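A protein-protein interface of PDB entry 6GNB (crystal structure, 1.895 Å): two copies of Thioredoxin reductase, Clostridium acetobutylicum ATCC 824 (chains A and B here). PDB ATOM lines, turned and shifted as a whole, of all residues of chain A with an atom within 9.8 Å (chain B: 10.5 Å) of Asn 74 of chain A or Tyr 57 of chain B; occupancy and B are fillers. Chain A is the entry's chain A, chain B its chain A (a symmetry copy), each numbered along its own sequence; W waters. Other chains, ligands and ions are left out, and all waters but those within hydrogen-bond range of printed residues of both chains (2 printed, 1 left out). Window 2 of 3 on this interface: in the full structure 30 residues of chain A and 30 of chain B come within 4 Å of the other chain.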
ATOM      1  N   ILE A  23       1.074  -8.125  -6.925  1.00  0.00           N
ATOM      2  CA  ILE A  23       2.346  -8.835  -6.772  1.00  0.00           C
ATOM      3  C   ILE A  23       2.629  -9.163  -5.313  1.00  0.00           C
ATOM      4  O   ILE A  23       3.430 -10.063  -5.028  1.00  0.00           O
ATOM      5  CB  ILE A  23       3.522  -8.093  -7.424  1.00  0.00           C
ATOM      6  CG1 ILE A  23       3.846  -6.781  -6.711  1.00  0.00           C
ATOM      7  CG2 ILE A  23       3.244  -7.843  -8.897  1.00  0.00           C
ATOM      8  CD1 ILE A  23       5.127  -6.127  -7.228  1.00  0.00           C
ATOM      9  N   LYS A  26      -0.016 -12.362  -4.290  1.00  0.00           N
ATOM     10  CA  LYS A  26       0.336 -13.696  -4.764  1.00  0.00           C
ATOM     11  C   LYS A  26       1.300 -14.365  -3.795  1.00  0.00           C
ATOM     12  O   LYS A  26       2.423 -14.726  -4.162  1.00  0.00           O
ATOM     13  CB  LYS A  26       0.931 -13.640  -6.169  1.00  0.00           C
ATOM     14  CG  LYS A  26      -0.086 -13.278  -7.224  1.00  0.00           C
ATOM     15  CD  LYS A  26       0.111 -14.089  -8.491  1.00  0.00           C
ATOM     16  CE  LYS A  26      -0.329 -15.526  -8.338  1.00  0.00           C
ATOM     17  NZ  LYS A  26      -0.266 -16.212  -9.654  1.00  0.00           N
ATOM     18  N   TYR A  53      10.434   8.070  -9.844  1.00  0.00           N
ATOM     19  CA  TYR A  53      10.215   6.670  -9.501  1.00  0.00           C
ATOM     20  C   TYR A  53      11.590   6.041  -9.281  1.00  0.00           C
ATOM     21  O   TYR A  53      12.327   5.777 -10.240  1.00  0.00           O
ATOM     22  CB  TYR A  53       9.400   5.960 -10.575  1.00  0.00           C
ATOM     23  CG  TYR A  53       8.884   4.610 -10.141  1.00  0.00           C
ATOM     24  CD1 TYR A  53       7.699   4.490  -9.476  1.00  0.00           C
ATOM     25  CD2 TYR A  53       9.568   3.443 -10.470  1.00  0.00           C
ATOM     26  CE1 TYR A  53       7.217   3.255  -9.073  1.00  0.00           C
ATOM     27  CE2 TYR A  53       9.097   2.182 -10.071  1.00  0.00           C
ATOM     28  CZ  TYR A  53       7.894   2.111  -9.363  1.00  0.00           C
ATOM     29  OH  TYR A  53       7.298   0.943  -8.906  1.00  0.00           O
ATOM     30  N   PHE A  56      14.364   4.109 -11.618  1.00  0.00           N
ATOM     31  CA  PHE A  56      14.047   4.225 -13.042  1.00  0.00           C
ATOM     32  C   PHE A  56      14.226   5.652 -13.544  1.00  0.00           C
ATOM     33  O   PHE A  56      13.402   6.180 -14.285  1.00  0.00           O
ATOM     34  CB  PHE A  56      12.618   3.775 -13.338  1.00  0.00           C
ATOM     35  CG  PHE A  56      12.401   2.288 -13.287  1.00  0.00           C
ATOM     36  CD1 PHE A  56      12.946   1.450 -14.242  1.00  0.00           C
ATOM     37  CD2 PHE A  56      11.605   1.740 -12.309  1.00  0.00           C
ATOM     38  CE1 PHE A  56      12.712   0.088 -14.187  1.00  0.00           C
ATOM     39  CE2 PHE A  56      11.363   0.396 -12.254  1.00  0.00           C
ATOM     40  CZ  PHE A  56      11.913  -0.432 -13.183  1.00  0.00           C
ATOM     41  N   GLU A  66       5.671  -1.012 -19.649  1.00  0.00           N
ATOM     42  CA  GLU A  66       6.112  -2.320 -20.116  1.00  0.00           C
ATOM     43  C   GLU A  66       6.845  -3.078 -19.013  1.00  0.00           C
ATOM     44  O   GLU A  66       6.683  -4.296 -18.881  1.00  0.00           O
ATOM     45  CB  GLU A  66       7.004  -2.157 -21.345  1.00  0.00           C
ATOM     46  CG  GLU A  66       7.598  -3.459 -21.887  1.00  0.00           C
ATOM     47  CD  GLU A  66       6.576  -4.494 -22.322  1.00  0.00           C
ATOM     48  OE1 GLU A  66       5.427  -4.127 -22.646  1.00  0.00           O
ATOM     49  OE2 GLU A  66       6.952  -5.693 -22.364  1.00  0.00           O
ATOM     50  N   LYS A  67       7.640  -2.381 -18.205  1.00  0.00           N
ATOM     51  CA  LYS A  67       8.278  -3.047 -17.078  1.00  0.00           C
ATOM     52  C   LYS A  67       7.224  -3.626 -16.140  1.00  0.00           C
ATOM     53  O   LYS A  67       7.393  -4.734 -15.608  1.00  0.00           O
ATOM     54  CB  LYS A  67       9.168  -2.063 -16.312  1.00  0.00           C
ATOM     55  CG  LYS A  67      10.274  -1.393 -17.158  1.00  0.00           C
ATOM     56  CD  LYS A  67      11.522  -2.203 -17.183  1.00  0.00           C
ATOM     57  CE  LYS A  67      12.684  -1.421 -17.766  1.00  0.00           C
ATOM     58  NZ  LYS A  67      13.667  -2.372 -18.304  1.00  0.00           N
ATOM     59  N   PHE A  68       6.126  -2.888 -15.921  1.00  0.00           N
ATOM     60  CA  PHE A  68       5.084  -3.383 -15.028  1.00  0.00           C
ATOM     61  C   PHE A  68       4.368  -4.580 -15.650  1.00  0.00           C
ATOM     62  O   PHE A  68       4.044  -5.555 -14.955  1.00  0.00           O
ATOM     63  CB  PHE A  68       4.076  -2.260 -14.732  1.00  0.00           C
ATOM     64  CG  PHE A  68       4.583  -1.144 -13.818  1.00  0.00           C
ATOM     65  CD1 PHE A  68       5.832  -1.173 -13.225  1.00  0.00           C
ATOM     66  CD2 PHE A  68       3.736  -0.063 -13.520  1.00  0.00           C
ATOM     67  CE1 PHE A  68       6.250  -0.137 -12.385  1.00  0.00           C
ATOM     68  CE2 PHE A  68       4.153   0.968 -12.693  1.00  0.00           C
ATOM     69  CZ  PHE A  68       5.409   0.929 -12.122  1.00  0.00           C
ATOM     70  N   LYS A  69       4.117  -4.515 -16.956  1.00  0.00           N
ATOM     71  CA  LYS A  69       3.492  -5.634 -17.649  1.00  0.00           C
ATOM     72  C   LYS A  69       4.354  -6.892 -17.563  1.00  0.00           C
ATOM     73  O   LYS A  69       3.843  -7.994 -17.330  1.00  0.00           O
ATOM     74  CB  LYS A  69       3.230  -5.244 -19.100  1.00  0.00           C
ATOM     75  CG  LYS A  69       2.502  -6.295 -19.900  1.00  0.00           C
ATOM     76  CD  LYS A  69       1.235  -6.774 -19.219  1.00  0.00           C
ATOM     77  CE  LYS A  69       0.308  -7.482 -20.194  1.00  0.00           C
ATOM     78  NZ  LYS A  69       1.027  -8.481 -21.034  1.00  0.00           N
ATOM     79  N   GLU A  70       5.659  -6.754 -17.762  1.00  0.00           N
ATOM     80  CA  GLU A  70       6.505  -7.938 -17.717  1.00  0.00           C
ATOM     81  C   GLU A  70       6.562  -8.512 -16.309  1.00  0.00           C
ATOM     82  O   GLU A  70       6.601  -9.737 -16.140  1.00  0.00           O
ATOM     83  CB  GLU A  70       7.885  -7.595 -18.263  1.00  0.00           C
ATOM     84  CG  GLU A  70       7.800  -7.265 -19.741  1.00  0.00           C
ATOM     85  CD  GLU A  70       9.143  -7.138 -20.414  1.00  0.00           C
ATOM     86  OE1 GLU A  70      10.140  -7.668 -19.882  1.00  0.00           O
ATOM     87  OE2 GLU A  70       9.186  -6.501 -21.484  1.00  0.00           O
ATOM     88  N   HIS A  71       6.499  -7.648 -15.288  1.00  0.00           N
ATOM     89  CA  HIS A  71       6.482  -8.125 -13.914  1.00  0.00           C
ATOM     90  C   HIS A  71       5.265  -9.006 -13.665  1.00  0.00           C
ATOM     91  O   HIS A  71       5.391 -10.131 -13.175  1.00  0.00           O
ATOM     92  CB  HIS A  71       6.461  -6.917 -12.980  1.00  0.00           C
ATOM     93  CG  HIS A  71       6.922  -7.207 -11.591  1.00  0.00           C
ATOM     94  ND1 HIS A  71       6.550  -8.325 -10.878  1.00  0.00           N
ATOM     95  CD2 HIS A  71       7.714  -6.488 -10.769  1.00  0.00           C
ATOM     96  CE1 HIS A  71       7.118  -8.290  -9.686  1.00  0.00           C
ATOM     97  NE2 HIS A  71       7.828  -7.187  -9.601  1.00  0.00           N
ATOM     98  N   ILE A  72       4.066  -8.509 -13.987  1.00  0.00           N
ATOM     99  CA  ILE A  72       2.880  -9.303 -13.672  1.00  0.00           C
ATOM    100  C   ILE A  72       2.851 -10.571 -14.511  1.00  0.00           C
ATOM    101  O   ILE A  72       2.451 -11.636 -14.027  1.00  0.00           O
ATOM    102  CB  ILE A  72       1.574  -8.483 -13.753  1.00  0.00           C
ATOM    103  CG1 ILE A  72       1.312  -7.924 -15.151  1.00  0.00           C
ATOM    104  CG2 ILE A  72       1.608  -7.367 -12.720  1.00  0.00           C
ATOM    105  CD1 ILE A  72      -0.087  -7.304 -15.279  1.00  0.00           C
ATOM    106  N   ASP A  73       3.290 -10.483 -15.766  1.00  0.00           N
ATOM    107  CA  ASP A  73       3.367 -11.665 -16.615  1.00  0.00           C
ATOM    108  C   ASP A  73       4.321 -12.699 -16.028  1.00  0.00           C
ATOM    109  O   ASP A  73       4.002 -13.893 -15.987  1.00  0.00           O
ATOM    110  CB  ASP A  73       3.803 -11.256 -18.021  1.00  0.00           C
ATOM    111  CG  ASP A  73       2.736 -10.444 -18.756  1.00  0.00           C
ATOM    112  OD1 ASP A  73       1.594 -10.333 -18.251  1.00  0.00           O
ATOM    113  OD2 ASP A  73       3.047  -9.913 -19.843  1.00  0.00           O
ATOM    114  N   ASN A  74       5.484 -12.262 -15.537  1.00  0.00           N
ATOM    115  CA  ASN A  74       6.396 -13.199 -14.898  1.00  0.00           C
ATOM    116  C   ASN A  74       5.777 -13.871 -13.677  1.00  0.00           C
ATOM    117  O   ASN A  74       6.177 -14.986 -13.325  1.00  0.00           O
ATOM    118  CB  ASN A  74       7.694 -12.496 -14.495  1.00  0.00           C
ATOM    119  CG  ASN A  74       8.713 -12.455 -15.622  1.00  0.00           C
ATOM    120  OD1 ASN A  74       9.220 -11.393 -15.982  1.00  0.00           O
ATOM    121  ND2 ASN A  74       9.023 -13.618 -16.178  1.00  0.00           N
ATOM    122  N   MET A  75       4.846 -13.214 -12.989  1.00  0.00           N
ATOM    123  CA  MET A  75       4.214 -13.794 -11.811  1.00  0.00           C
ATOM    124  C   MET A  75       2.866 -14.440 -12.106  1.00  0.00           C
ATOM    125  O   MET A  75       2.142 -14.785 -11.165  1.00  0.00           O
ATOM    126  CB  MET A  75       4.052 -12.735 -10.732  1.00  0.00           C
ATOM    127  CG  MET A  75       5.385 -12.230 -10.250  1.00  0.00           C
ATOM    128  SD  MET A  75       5.256 -11.034  -8.927  1.00  0.00           S
ATOM    129  CE  MET A  75       4.928 -12.105  -7.532  1.00  0.00           C
ATOM    130  N   GLY A  76       2.508 -14.606 -13.372  1.00  0.00           N
ATOM    131  CA  GLY A  76       1.266 -15.278 -13.699  1.00  0.00           C
ATOM    132  C   GLY A  76       0.026 -14.519 -13.286  1.00  0.00           C
ATOM    133  O   GLY A  76      -0.999 -15.133 -12.985  1.00  0.00           O
ATOM    134  N   ILE A  77       0.104 -13.193 -13.235  1.00  0.00           N
ATOM    135  CA  ILE A  77      -1.022 -12.337 -12.889  1.00  0.00           C
ATOM    136  C   ILE A  77      -1.609 -11.822 -14.186  1.00  0.00           C
ATOM    137  O   ILE A  77      -0.909 -11.177 -14.972  1.00  0.00           O
ATOM    138  CB  ILE A  77      -0.561 -11.161 -12.020  1.00  0.00           C
ATOM    139  CG1 ILE A  77      -0.126 -11.676 -10.653  1.00  0.00           C
ATOM    140  CG2 ILE A  77      -1.663 -10.109 -11.887  1.00  0.00           C
ATOM    141  CD1 ILE A  77       0.653 -10.679  -9.837  1.00  0.00           C
ATOM    142  N   GLN A  78      -2.889 -12.086 -14.399  1.00  0.00           N
ATOM    143  CA  GLN A  78      -3.606 -11.584 -15.561  1.00  0.00           C
ATOM    144  C   GLN A  78      -4.605 -10.528 -15.119  1.00  0.00           C
ATOM    145  O   GLN A  78      -5.063 -10.521 -13.975  1.00  0.00           O
ATOM    146  CB  GLN A  78      -4.344 -12.712 -16.281  1.00  0.00           C
ATOM    147  CG  GLN A  78      -3.426 -13.753 -16.900  1.00  0.00           C
ATOM    148  CD  GLN A  78      -2.966 -14.801 -15.905  1.00  0.00           C
ATOM    149  OE1 GLN A  78      -3.689 -15.148 -14.969  1.00  0.00           O
ATOM    150  NE2 GLN A  78      -1.755 -15.311 -16.103  1.00  0.00           N
ATOM    151  N   PRO B  48      18.563 -11.128  -1.311  1.00  0.00           N
ATOM    152  CA  PRO B  48      19.016 -12.009  -2.409  1.00  0.00           C
ATOM    153  C   PRO B  48      18.327 -11.850  -3.772  1.00  0.00           C
ATOM    154  O   PRO B  48      18.987 -11.456  -4.741  1.00  0.00           O
ATOM    155  CB  PRO B  48      18.814 -13.418  -1.834  1.00  0.00           C
ATOM    156  CG  PRO B  48      17.759 -13.261  -0.794  1.00  0.00           C
ATOM    157  CD  PRO B  48      17.871 -11.873  -0.245  1.00  0.00           C
ATOM    158  N   VAL B  49      17.050 -12.237  -3.893  1.00  0.00           N
ATOM    159  CA  VAL B  49      16.203 -11.911  -5.032  1.00  0.00           C
ATOM    160  C   VAL B  49      14.994 -11.151  -4.509  1.00  0.00           C
ATOM    161  O   VAL B  49      14.443 -11.504  -3.465  1.00  0.00           O
ATOM    162  CB  VAL B  49      15.784 -13.187  -5.776  1.00  0.00           C
ATOM    163  CG1 VAL B  49      15.040 -14.128  -4.838  1.00  0.00           C
ATOM    164  CG2 VAL B  49      14.937 -12.840  -6.999  1.00  0.00           C
ATOM    165  N   ILE B  50      14.575 -10.111  -5.232  1.00  0.00           N
ATOM    166  CA  ILE B  50      13.438  -9.277  -4.844  1.00  0.00           C
ATOM    167  C   ILE B  50      12.403  -9.365  -5.951  1.00  0.00           C
ATOM    168  O   ILE B  50      12.681  -8.988  -7.096  1.00  0.00           O
ATOM    169  CB  ILE B  50      13.854  -7.817  -4.626  1.00  0.00           C
ATOM    170  CG1 ILE B  50      14.913  -7.734  -3.528  1.00  0.00           C
ATOM    171  CG2 ILE B  50      12.631  -6.936  -4.310  1.00  0.00           C
ATOM    172  CD1 ILE B  50      15.690  -6.452  -3.556  1.00  0.00           C
ATOM    173  N   ASN B  51      11.208  -9.839  -5.611  1.00  0.00           N
ATOM    174  CA  ASN B  51      10.130  -9.980  -6.578  1.00  0.00           C
ATOM    175  C   ASN B  51       8.922  -9.108  -6.295  1.00  0.00           C
ATOM    176  O   ASN B  51       7.953  -9.167  -7.053  1.00  0.00           O
ATOM    177  CB  ASN B  51       9.686 -11.444  -6.683  1.00  0.00           C
ATOM    178  CG  ASN B  51      10.792 -12.339  -7.169  1.00  0.00           C
ATOM    179  OD1 ASN B  51      11.575 -11.948  -8.031  1.00  0.00           O
ATOM    180  ND2 ASN B  51      10.865 -13.547  -6.627  1.00  0.00           N
ATOM    181  N   ASN B  52       8.945  -8.295  -5.244  1.00  0.00           N
ATOM    182  CA  ASN B  52       7.804  -7.463  -4.894  1.00  0.00           C
ATOM    183  C   ASN B  52       8.129  -5.982  -4.972  1.00  0.00           C
ATOM    184  O   ASN B  52       7.486  -5.180  -4.285  1.00  0.00           O
ATOM    185  CB  ASN B  52       7.261  -7.845  -3.517  1.00  0.00           C
ATOM    186  CG  ASN B  52       8.212  -7.492  -2.404  1.00  0.00           C
ATOM    187  OD1 ASN B  52       9.358  -7.135  -2.643  1.00  0.00           O
ATOM    188  ND2 ASN B  52       7.719  -7.552  -1.164  1.00  0.00           N
ATOM    189  N   TYR B  53       9.107  -5.600  -5.771  1.00  0.00           N
ATOM    190  CA  TYR B  53       9.334  -4.205  -6.125  1.00  0.00           C
ATOM    191  C   TYR B  53       8.926  -4.040  -7.588  1.00  0.00           C
ATOM    192  O   TYR B  53       9.644  -4.474  -8.499  1.00  0.00           O
ATOM    193  CB  TYR B  53      10.778  -3.797  -5.860  1.00  0.00           C
ATOM    194  CG  TYR B  53      10.999  -2.305  -5.914  1.00  0.00           C
ATOM    195  CD1 TYR B  53      10.809  -1.524  -4.811  1.00  0.00           C
ATOM    196  CD2 TYR B  53      11.472  -1.693  -7.072  1.00  0.00           C
ATOM    197  CE1 TYR B  53      11.009  -0.154  -4.851  1.00  0.00           C
ATOM    198  CE2 TYR B  53      11.680  -0.306  -7.134  1.00  0.00           C
ATOM    199  CZ  TYR B  53      11.441   0.457  -5.987  1.00  0.00           C
ATOM    200  OH  TYR B  53      11.605   1.832  -5.889  1.00  0.00           O
ATOM    201  N   LEU B  54       7.789  -3.377  -7.789  1.00  0.00           N
ATOM    202  CA  LEU B  54       7.094  -3.390  -9.070  1.00  0.00           C
ATOM    203  C   LEU B  54       7.954  -2.758 -10.159  1.00  0.00           C
ATOM    204  O   LEU B  54       8.412  -1.615 -10.034  1.00  0.00           O
ATOM    205  CB  LEU B  54       5.767  -2.655  -8.947  1.00  0.00           C
ATOM    206  CG  LEU B  54       4.878  -2.695 -10.201  1.00  0.00           C
ATOM    207  CD1 LEU B  54       4.423  -4.113 -10.568  1.00  0.00           C
ATOM    208  CD2 LEU B  54       3.685  -1.770 -10.025  1.00  0.00           C
ATOM    209  N   GLY B  55       8.146  -3.500 -11.240  1.00  0.00           N
ATOM    210  CA  GLY B  55       9.003  -3.096 -12.331  1.00  0.00           C
ATOM    211  C   GLY B  55      10.386  -3.711 -12.328  1.00  0.00           C
ATOM    212  O   GLY B  55      11.082  -3.624 -13.352  1.00  0.00           O
ATOM    213  N   PHE B  56      10.803  -4.341 -11.232  1.00  0.00           N
ATOM    214  CA  PHE B  56      12.132  -4.943 -11.108  1.00  0.00           C
ATOM    215  C   PHE B  56      12.049  -6.416 -10.730  1.00  0.00           C
ATOM    216  O   PHE B  56      12.787  -6.903  -9.878  1.00  0.00           O
ATOM    217  CB  PHE B  56      12.983  -4.216 -10.070  1.00  0.00           C
ATOM    218  CG  PHE B  56      13.500  -2.872 -10.505  1.00  0.00           C
ATOM    219  CD1 PHE B  56      14.463  -2.759 -11.491  1.00  0.00           C
ATOM    220  CD2 PHE B  56      13.055  -1.728  -9.887  1.00  0.00           C
ATOM    221  CE1 PHE B  56      14.939  -1.513 -11.857  1.00  0.00           C
ATOM    222  CE2 PHE B  56      13.527  -0.495 -10.239  1.00  0.00           C
ATOM    223  CZ  PHE B  56      14.462  -0.380 -11.220  1.00  0.00           C
ATOM    224  N   TYR B  57      11.151  -7.167 -11.343  1.00  0.00           N
ATOM    225  CA  TYR B  57      11.033  -8.579 -10.997  1.00  0.00           C
ATOM    226  C   TYR B  57      12.369  -9.303 -11.115  1.00  0.00           C
ATOM    227  O   TYR B  57      13.076  -9.181 -12.124  1.00  0.00           O
ATOM    228  CB  TYR B  57      10.008  -9.246 -11.908  1.00  0.00           C
ATOM    229  CG  TYR B  57       9.886 -10.727 -11.667  1.00  0.00           C
ATOM    230  CD1 TYR B  57       9.098 -11.210 -10.640  1.00  0.00           C
ATOM    231  CD2 TYR B  57      10.570 -11.645 -12.457  1.00  0.00           C
ATOM    232  CE1 TYR B  57       8.974 -12.572 -10.410  1.00  0.00           C
ATOM    233  CE2 TYR B  57      10.461 -13.004 -12.231  1.00  0.00           C
ATOM    234  CZ  TYR B  57       9.663 -13.460 -11.200  1.00  0.00           C
ATOM    235  OH  TYR B  57       9.554 -14.809 -10.962  1.00  0.00           O
ATOM    236  N   GLY B  58      12.703 -10.074 -10.078  1.00  0.00           N
ATOM    237  CA  GLY B  58      13.877 -10.927 -10.104  1.00  0.00           C
ATOM    238  C   GLY B  58      15.185 -10.221  -9.856  1.00  0.00           C
ATOM    239  O   GLY B  58      16.250 -10.843  -9.994  1.00  0.00           O
ATOM    240  N   ILE B  59      15.149  -8.942  -9.491  1.00  0.00           N
ATOM    241  CA  ILE B  59      16.383  -8.205  -9.258  1.00  0.00           C
ATOM    242  C   ILE B  59      17.026  -8.655  -7.954  1.00  0.00           C
ATOM    243  O   ILE B  59      16.355  -9.049  -6.994  1.00  0.00           O
ATOM    244  CB  ILE B  59      16.078  -6.695  -9.265  1.00  0.00           C
ATOM    245  CG1 ILE B  59      17.363  -5.888  -9.388  1.00  0.00           C
ATOM    246  CG2 ILE B  59      15.297  -6.269  -8.015  1.00  0.00           C
ATOM    247  CD1 ILE B  59      17.099  -4.460  -9.779  1.00  0.00           C
ATOM    248  N   ARG B  60      18.347  -8.620  -7.925  1.00  0.00           N
ATOM    249  CA  ARG B  60      19.089  -8.885  -6.706  1.00  0.00           C
ATOM    250  C   ARG B  60      19.245  -7.591  -5.913  1.00  0.00           C
ATOM    251  O   ARG B  60      19.284  -6.502  -6.486  1.00  0.00           O
ATOM    252  CB  ARG B  60      20.464  -9.453  -7.061  1.00  0.00           C
ATOM    253  CG  ARG B  60      20.385 -10.691  -7.947  1.00  0.00           C
ATOM    254  CD  ARG B  60      21.608 -10.876  -8.836  1.00  0.00           C
ATOM    255  NE  ARG B  60      22.790 -11.301  -8.098  1.00  0.00           N
ATOM    256  CZ  ARG B  60      23.907 -11.742  -8.672  1.00  0.00           C
ATOM    257  NH1 ARG B  60      24.940 -12.109  -7.926  1.00  0.00           N
ATOM    258  NH2 ARG B  60      23.992 -11.822  -9.995  1.00  0.00           N
ATOM    259  N   GLY B  61      19.354  -7.728  -4.589  1.00  0.00           N
ATOM    260  CA  GLY B  61      19.437  -6.559  -3.725  1.00  0.00           C
ATOM    261  C   GLY B  61      20.533  -5.590  -4.124  1.00  0.00           C
ATOM    262  O   GLY B  61      20.320  -4.377  -4.186  1.00  0.00           O
ATOM    263  N   GLU B  63      21.875  -5.290  -7.005  1.00  0.00           N
ATOM    264  CA  GLU B  63      21.518  -4.691  -8.284  1.00  0.00           C
ATOM    265  C   GLU B  63      20.550  -3.531  -8.094  1.00  0.00           C
ATOM    266  O   GLU B  63      20.688  -2.481  -8.734  1.00  0.00           O
ATOM    267  CB  GLU B  63      20.893  -5.756  -9.184  1.00  0.00           C
ATOM    268  CG  GLU B  63      21.904  -6.744  -9.710  1.00  0.00           C
ATOM    269  CD  GLU B  63      21.269  -7.859 -10.517  1.00  0.00           C
ATOM    270  OE1 GLU B  63      20.079  -8.163 -10.289  1.00  0.00           O
ATOM    271  OE2 GLU B  63      21.955  -8.439 -11.390  1.00  0.00           O
ATOM    272  N   LEU B  64      19.556  -3.705  -7.224  1.00  0.00           N
ATOM    273  CA  LEU B  64      18.618  -2.622  -6.962  1.00  0.00           C
ATOM    274  C   LEU B  64      19.337  -1.473  -6.277  1.00  0.00           C
ATOM    275  O   LEU B  64      19.106  -0.301  -6.596  1.00  0.00           O
ATOM    276  CB  LEU B  64      17.474  -3.148  -6.104  1.00  0.00           C
ATOM    277  CG  LEU B  64      16.319  -2.190  -5.809  1.00  0.00           C
ATOM    278  CD1 LEU B  64      15.651  -1.740  -7.103  1.00  0.00           C
ATOM    279  CD2 LEU B  64      15.315  -2.887  -4.932  1.00  0.00           C
ATOM    280  N   LYS B  67      20.899   0.529  -8.981  1.00  0.00           N
ATOM    281  CA  LYS B  67      19.920   1.360  -9.669  1.00  0.00           C
ATOM    282  C   LYS B  67      19.600   2.598  -8.840  1.00  0.00           C
ATOM    283  O   LYS B  67      19.443   3.701  -9.387  1.00  0.00           O
ATOM    284  CB  LYS B  67      18.637   0.564  -9.929  1.00  0.00           C
ATOM    285  CG  LYS B  67      18.829  -0.730 -10.753  1.00  0.00           C
ATOM    286  CD  LYS B  67      18.739  -0.475 -12.216  1.00  0.00           C
ATOM    287  CE  LYS B  67      18.642  -1.769 -13.003  1.00  0.00           C
ATOM    288  NZ  LYS B  67      19.137  -1.528 -14.366  1.00  0.00           N
ATOM    289  N   MET B 267       8.447  -0.943  -1.207  1.00  0.00           N
ATOM    290  CA  MET B 267       7.440  -0.073  -1.820  1.00  0.00           C
ATOM    291  C   MET B 267       6.768   0.830  -0.790  1.00  0.00           C
ATOM    292  O   MET B 267       6.581   2.021  -1.034  1.00  0.00           O
ATOM    293  CB  MET B 267       6.446  -0.883  -2.651  1.00  0.00           C
ATOM    294  CG  MET B 267       7.127  -1.549  -3.841  1.00  0.00           C
ATOM    295  SD  MET B 267       6.067  -1.855  -5.266  1.00  0.00           S
ATOM    296  CE  MET B 267       4.898  -3.013  -4.557  1.00  0.00           C
HETATM  297  O   HOH W   1       9.701  -6.350 -14.178  1.00  0.00           O
HETATM  298  O   HOH W   2      10.722  -7.002  -7.666  1.00  0.00           O
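Among the printed residues, merely in contact across the chains: Ile 23 of chain A with Asn 52 of chain B, Ile 23 of chain A with Leu 54 of chain B, Phe 56 of chain A with Gly 55 of chain B, Phe 56 of chain A with Phe 56 of chain B, Lys 67 of chain A with Gly 55 of chain B, Phe 68 of chain A with Leu 54 of chain B, Phe 68 of chain A with Gly 55 of chain B, His 71 of chain A with Leu 54 of chain B, His 71 of chain A with Gly 55 of chain B, His 71 of chain A with Phe 56 of chain B, His 71 of chain A with Tyr 57 of chain B, Asn 74 of chain A with Tyr 57 of chain B and Met 75 of chain A with Tyr 57 of chain B.
Phe 56 of chain A touches its own counterpart, Phe 56 of chain B. Positions printed for both chains: 53, 56 and 67.
The side-chain hydroxyl of Tyr 53 of chain A sits at hydrogen-bond distance from the backbone carbonyl oxygen of Leu 54 of chain B (3.0 Å). The backbone carbonyl oxygen (O) of Asn 51 of chain B sits close to a ring nitrogen (NE2) of His 71 of chain A (3.2 Å). The backbone carbonyl oxygen (O) of Asn 51 of chain B sits close to the side-chain sulfur (SD) of Met 75 of chain A (3.8 Å). NE2 of His 71 of chain A sits at hydrogen-bond distance from O of Tyr 53 of chain B (3.4 Å).
Of the printed residues of chain B, Phe 56 of chain A touches Gly 55 (3.3 Å) and Phe 56 (3.1 Å). Of the printed residues of chain B, Lys 67 of chain A touches Gly 55 (3.9 Å). His 71 of chain A touches just these residues of chain B: Asn 51, Tyr 53, Leu 54, Gly 55, Phe 56 and Tyr 57. Asn 74 of chain A touches just one residue of chain B: Tyr 57 (3.6 Å). Met 75 of chain A touches two residues of chain B. Of the printed residues of chain A, Phe 56 of chain B touches Phe 56 and His 71. Tyr 57 of chain B touches just these residues of chain A: His 71, Asn 74 and Met 75. Gly 58 of chain B touches none of the printed residues of chain A.
Of the 17 printed residues of chain A, 8 touch a printed residue of chain B. Hydrophobic or aromatic side chains of chain A within 4 Å of the printed part of chain B: Ile 23, Tyr 53, Phe 56, Phe 68, His 71 and Met 75. Of the 18 printed residues of chain B, 7 touch a printed residue of chain A. Printed residues of chain B that touch a printed residue of chain A: Asn 51, Asn 52, Tyr 53, Leu 54, Gly 55, Phe 56 and Tyr 57. Hydrophobic or aromatic side chains of chain B within 4 Å of the printed part of chain A: Leu 54, Phe 56 and Tyr 57. Among the printed residues, no Asp or Glu carboxylate lies within 4 Å of a Lys or Arg side-chain nitrogen of the other chain.
Water W2 lies within hydrogen-bond range of the backbone carbonyl oxygen (O) of Ile 50 of chain B (2.8 Å), the backbone NH (N) of Tyr 53 of chain B (2.9 Å), the backbone carbonyl oxygen (O) of Phe 56 of chain B (3.0 Å), the backbone NH (N) of Asn 52 of chain B (3.3 Å) and a ring nitrogen (NE2) of His 71 of chain A (3.5 Å). Water W1 lies within hydrogen-bond range of the backbone carbonyl oxygen (O) of Lys 67 of chain A, the backbone carbonyl oxygen (O) of Gly 55 of chain B and the backbone NH (N) of Tyr 57 of chain B.
OD1 of Asn 51 of chain B is in hydrogen-bond range of N of Gly 58 of chain B (3.0 Å). NZ of Lys 26 of chain A lies within hydrogen-bond range of O of Met 75 of chain A (3.2 Å). O of Glu 70 of chain A lies close to OD1 of Asn 74 of chain A, at 3.1 Å. ND1 of His 71 of chain A sits close to SD of Met 75 of chain A (3.6 Å). N of Leu 54 of chain B sits at hydrogen-bond distance from SD of Met 267 of chain B (3.4 Å).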
